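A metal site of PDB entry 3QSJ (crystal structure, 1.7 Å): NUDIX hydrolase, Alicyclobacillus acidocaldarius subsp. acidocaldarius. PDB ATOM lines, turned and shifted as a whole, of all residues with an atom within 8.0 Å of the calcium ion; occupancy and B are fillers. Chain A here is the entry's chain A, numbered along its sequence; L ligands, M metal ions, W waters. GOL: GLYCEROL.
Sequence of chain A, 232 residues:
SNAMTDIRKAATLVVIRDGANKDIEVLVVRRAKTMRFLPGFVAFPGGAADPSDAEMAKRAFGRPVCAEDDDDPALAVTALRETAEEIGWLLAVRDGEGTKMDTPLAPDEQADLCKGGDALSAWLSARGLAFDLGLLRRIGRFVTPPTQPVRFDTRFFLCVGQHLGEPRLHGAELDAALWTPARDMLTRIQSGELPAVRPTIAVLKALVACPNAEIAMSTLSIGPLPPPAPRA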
ATOM      1  N   ALA A  11       5.333 -30.276  22.924  1.00  0.00           N
ATOM      2  CA  ALA A  11       5.976 -31.305  23.763  1.00  0.00           C
ATOM      3  C   ALA A  11       6.209 -30.744  25.104  1.00  0.00           C
ATOM      4  O   ALA A  11       6.347 -29.522  25.301  1.00  0.00           O
ATOM      5  CB  ALA A  11       7.307 -31.755  23.171  1.00  0.00           C
ATOM      6  N   VAL A  29       5.518 -25.851  36.973  1.00  0.00           N
ATOM      7  CA  VAL A  29       5.448 -24.389  36.854  1.00  0.00           C
ATOM      8  C   VAL A  29       3.997 -23.934  36.919  1.00  0.00           C
ATOM      9  O   VAL A  29       3.095 -24.728  36.665  1.00  0.00           O
ATOM     10  CB  VAL A  29       6.112 -23.903  35.550  1.00  0.00           C
ATOM     11  CG1 VAL A  29       7.615 -24.322  35.525  1.00  0.00           C
ATOM     12  CG2 VAL A  29       5.368 -24.411  34.310  1.00  0.00           C
ATOM     13  N   ARG A  31       1.378 -20.952  35.365  1.00  0.00           N
ATOM     14  CA  ARG A  31       1.112 -19.785  34.474  1.00  0.00           C
ATOM     15  C   ARG A  31       0.595 -18.609  35.277  1.00  0.00           C
ATOM     16  O   ARG A  31      -0.287 -18.766  36.119  1.00  0.00           O
ATOM     17  CB  ARG A  31       0.092 -20.161  33.392  1.00  0.00           C
ATOM     18  CG  ARG A  31       0.632 -21.256  32.506  1.00  0.00           C
ATOM     19  CD  ARG A  31      -0.457 -21.814  31.611  1.00  0.00           C
ATOM     20  NE  ARG A  31      -0.760 -20.866  30.550  1.00  0.00           N
ATOM     21  CZ  ARG A  31      -0.071 -20.767  29.414  1.00  0.00           C
ATOM     22  NH1 ARG A  31       0.991 -21.541  29.204  1.00  0.00           N
ATOM     23  NH2 ARG A  31      -0.419 -19.878  28.507  1.00  0.00           N
ATOM     24  N   PHE A  44       3.820 -28.858  33.440  1.00  0.00           N
ATOM     25  CA  PHE A  44       5.251 -29.109  33.353  1.00  0.00           C
ATOM     26  C   PHE A  44       5.773 -28.169  32.251  1.00  0.00           C
ATOM     27  O   PHE A  44       5.001 -27.713  31.400  1.00  0.00           O
ATOM     28  CB  PHE A  44       5.520 -30.569  32.942  1.00  0.00           C
ATOM     29  CG  PHE A  44       4.812 -31.573  33.835  1.00  0.00           C
ATOM     30  CD1 PHE A  44       5.138 -31.682  35.188  1.00  0.00           C
ATOM     31  CD2 PHE A  44       3.810 -32.395  33.320  1.00  0.00           C
ATOM     32  CE1 PHE A  44       4.444 -32.564  36.020  1.00  0.00           C
ATOM     33  CE2 PHE A  44       3.107 -33.274  34.155  1.00  0.00           C
ATOM     34  CZ  PHE A  44       3.421 -33.348  35.500  1.00  0.00           C
ATOM     35  N   PRO A  45       7.078 -27.911  32.201  1.00  0.00           N
ATOM     36  CA  PRO A  45       7.621 -27.066  31.132  1.00  0.00           C
ATOM     37  C   PRO A  45       7.352 -27.664  29.766  1.00  0.00           C
ATOM     38  O   PRO A  45       7.368 -28.900  29.626  1.00  0.00           O
ATOM     39  CB  PRO A  45       9.159 -27.048  31.432  1.00  0.00           C
ATOM     40  CG  PRO A  45       9.233 -27.293  32.926  1.00  0.00           C
ATOM     41  CD  PRO A  45       8.144 -28.351  33.145  1.00  0.00           C
ATOM     42  N   GLY A  46       7.050 -26.825  28.791  1.00  0.00           N
ATOM     43  CA  GLY A  46       6.742 -27.351  27.456  1.00  0.00           C
ATOM     44  C   GLY A  46       6.244 -26.292  26.521  1.00  0.00           C
ATOM     45  O   GLY A  46       6.179 -25.109  26.883  1.00  0.00           O
ATOM     46  N   GLY A  47       5.887 -26.675  25.324  1.00  0.00           N
ATOM     47  CA  GLY A  47       5.353 -25.689  24.399  1.00  0.00           C
ATOM     48  C   GLY A  47       5.378 -26.195  22.989  1.00  0.00           C
ATOM     49  O   GLY A  47       5.691 -27.360  22.717  1.00  0.00           O
ATOM     50  N   ALA A  48       5.046 -25.298  22.086  1.00  0.00           N
ATOM     51  CA  ALA A  48       4.862 -25.603  20.668  1.00  0.00           C
ATOM     52  C   ALA A  48       6.172 -25.894  20.037  1.00  0.00           C
ATOM     53  O   ALA A  48       7.204 -25.240  20.325  1.00  0.00           O
ATOM     54  CB  ALA A  48       4.159 -24.419  19.959  1.00  0.00           C
ATOM     55  N   THR A  78      12.048 -30.212  21.340  1.00  0.00           N
ATOM     56  CA  THR A  78      11.065 -29.157  21.675  1.00  0.00           C
ATOM     57  C   THR A  78      10.950 -29.123  23.190  1.00  0.00           C
ATOM     58  O   THR A  78      11.013 -28.067  23.783  1.00  0.00           O
ATOM     59  CB  THR A  78       9.685 -29.474  21.022  1.00  0.00           C
ATOM     60  OG1 THR A  78       9.856 -29.506  19.592  1.00  0.00           O
ATOM     61  CG2 THR A  78       8.572 -28.485  21.505  1.00  0.00           C
ATOM     62  N   ALA A  79      10.773 -30.279  23.808  1.00  0.00           N
ATOM     63  CA  ALA A  79      10.607 -30.350  25.267  1.00  0.00           C
ATOM     64  C   ALA A  79      11.823 -29.806  26.034  1.00  0.00           C
ATOM     65  O   ALA A  79      11.650 -29.026  26.980  1.00  0.00           O
ATOM     66  CB  ALA A  79      10.289 -31.776  25.677  1.00  0.00           C
ATOM     67  N   ARG A  81      14.166 -27.746  24.857  1.00  0.00           N
ATOM     68  CA  ARG A  81      14.323 -26.307  24.612  1.00  0.00           C
ATOM     69  C   ARG A  81      13.375 -25.461  25.496  1.00  0.00           C
ATOM     70  O   ARG A  81      13.790 -24.442  26.032  1.00  0.00           O
ATOM     71  CB  ARG A  81      14.055 -25.971  23.115  1.00  0.00           C
ATOM     72  CG  ARG A  81      14.041 -24.421  22.844  1.00  0.00           C
ATOM     73  CD  ARG A  81      13.732 -24.058  21.361  1.00  0.00           C
ATOM     74  NE  ARG A  81      12.536 -24.760  20.873  1.00  0.00           N
ATOM     75  CZ  ARG A  81      11.284 -24.468  21.207  1.00  0.00           C
ATOM     76  NH1 ARG A  81      11.015 -23.447  22.041  1.00  0.00           N
ATOM     77  NH2 ARG A  81      10.272 -25.186  20.709  1.00  0.00           N
ATOM     78  N   GLU A  82      12.097 -25.855  25.547  1.00  0.00           N
ATOM     79  CA  GLU A  82      11.042 -25.146  26.293  1.00  0.00           C
ATOM     80  C   GLU A  82      11.387 -25.165  27.783  1.00  0.00           C
ATOM     81  O   GLU A  82      11.235 -24.148  28.480  1.00  0.00           O
ATOM     82  CB  GLU A  82       9.701 -25.836  26.039  1.00  0.00           C
ATOM     83  CG  GLU A  82       9.150 -25.584  24.636  1.00  0.00           C
ATOM     84  CD  GLU A  82       8.559 -24.191  24.393  1.00  0.00           C
ATOM     85  OE1 GLU A  82       8.147 -23.540  25.387  1.00  0.00           O
ATOM     86  OE2 GLU A  82       8.411 -23.800  23.211  1.00  0.00           O
ATOM     87  N   THR A  83      11.979 -26.283  28.250  1.00  0.00           N
ATOM     88  CA  THR A  83      12.408 -26.394  29.637  1.00  0.00           C
ATOM     89  C   THR A  83      13.536 -25.384  29.928  1.00  0.00           C
ATOM     90  O   THR A  83      13.526 -24.726  30.981  1.00  0.00           O
ATOM     91  CB  THR A  83      12.841 -27.850  29.951  1.00  0.00           C
ATOM     92  OG1 THR A  83      11.697 -28.697  29.749  1.00  0.00           O
ATOM     93  CG2 THR A  83      13.320 -27.998  31.386  1.00  0.00           C
ATOM     94  N   GLU A  85      14.116 -22.614  28.422  1.00  0.00           N
ATOM     95  CA  GLU A  85      13.535 -21.256  28.419  1.00  0.00           C
ATOM     96  C   GLU A  85      12.820 -20.968  29.715  1.00  0.00           C
ATOM     97  O   GLU A  85      12.903 -19.863  30.219  1.00  0.00           O
ATOM     98  CB  GLU A  85      12.501 -21.125  27.284  1.00  0.00           C
ATOM     99  CG  GLU A  85      13.106 -21.197  25.894  1.00  0.00           C
ATOM    100  CD  GLU A  85      12.074 -21.233  24.784  1.00  0.00           C
ATOM    101  OE1 GLU A  85      10.868 -21.065  25.100  1.00  0.00           O
ATOM    102  OE2 GLU A  85      12.446 -21.440  23.614  1.00  0.00           O
ATOM    103  N   GLU A  86      12.071 -21.955  30.242  1.00  0.00           N
ATOM    104  CA  GLU A  86      11.206 -21.729  31.389  1.00  0.00           C
ATOM    105  C   GLU A  86      11.913 -21.755  32.728  1.00  0.00           C
ATOM    106  O   GLU A  86      11.614 -20.914  33.580  1.00  0.00           O
ATOM    107  CB  GLU A  86      10.061 -22.769  31.325  1.00  0.00           C
ATOM    108  CG  GLU A  86       9.091 -22.463  30.202  1.00  0.00           C
ATOM    109  CD  GLU A  86       7.951 -23.451  30.185  1.00  0.00           C
ATOM    110  OE1 GLU A  86       7.367 -23.714  31.261  1.00  0.00           O
ATOM    111  OE2 GLU A  86       7.597 -23.902  29.070  1.00  0.00           O
ATOM    112  N   GLU A 173       5.710 -14.735  32.276  1.00  0.00           N
ATOM    113  CA  GLU A 173       4.760 -15.771  31.880  1.00  0.00           C
ATOM    114  C   GLU A 173       4.392 -16.754  32.954  1.00  0.00           C
ATOM    115  O   GLU A 173       3.209 -17.125  33.050  1.00  0.00           O
ATOM    116  CB  GLU A 173       5.244 -16.464  30.610  1.00  0.00           C
ATOM    117  CG  GLU A 173       4.749 -15.645  29.423  1.00  0.00           C
ATOM    118  CD  GLU A 173       5.569 -15.615  28.162  1.00  0.00           C
ATOM    119  OE1 GLU A 173       5.774 -14.502  27.633  1.00  0.00           O
ATOM    120  OE2 GLU A 173       5.941 -16.700  27.661  1.00  0.00           O
ATOM    121  N   LEU A 174       5.391 -17.145  33.791  1.00  0.00           N
ATOM    122  CA  LEU A 174       5.155 -18.101  34.883  1.00  0.00           C
ATOM    123  C   LEU A 174       5.296 -17.337  36.189  1.00  0.00           C
ATOM    124  O   LEU A 174       6.160 -16.482  36.279  1.00  0.00           O
ATOM    125  CB  LEU A 174       6.221 -19.247  34.827  1.00  0.00           C
ATOM    126  CG  LEU A 174       6.220 -20.042  33.530  1.00  0.00           C
ATOM    127  CD1 LEU A 174       7.336 -21.050  33.494  1.00  0.00           C
ATOM    128  CD2 LEU A 174       4.827 -20.679  33.293  1.00  0.00           C
HETATM  129  C1  GOL L   1       4.791 -19.674  29.708  1.00  0.00           C
HETATM  130  O1  GOL L   1       4.703 -18.881  28.538  1.00  0.00           O
HETATM  131  C2  GOL L   1       5.415 -21.041  29.444  1.00  0.00           C
HETATM  132  O2  GOL L   1       6.461 -20.895  28.535  1.00  0.00           O
HETATM  133  C3  GOL L   1       4.381 -21.952  28.821  1.00  0.00           C
HETATM  134  O3  GOL L   1       4.965 -23.140  28.296  1.00  0.00           O
HETATM  135 CA    CA M   1       6.808 -22.895  27.216  1.00  0.00          CA
HETATM  136  O   HOH W   1       5.638 -21.893  25.479  1.00  0.00           O
HETATM  137  O   HOH W   2       8.717 -21.324  27.029  1.00  0.00           O
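The guanidinium group (NH1) of Arg 81 lies within salt-bridge range of the side-chain carboxylate (OE2) of Glu 82 (2.9 Å).
O3 of the ligand binds the calcium ion (2.2 Å). OE2 of Glu 86 is bound to the calcium ion. The calcium ion is bound by water W1. O of Gly 46 is bound to the calcium ion. The calcium ion is bound by OE1 of Glu 82, 2.4 Å away. The calcium ion is bound by O2 of the ligand. Water W2 binds the calcium ion (2.5 Å).
Three residues have an atom within 4 Å of the calcium ion: Gly 46, Glu 82 and Glu 86. The nearest printed residue that does not touch the calcium ion is Gly 47 (4.2 Å).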
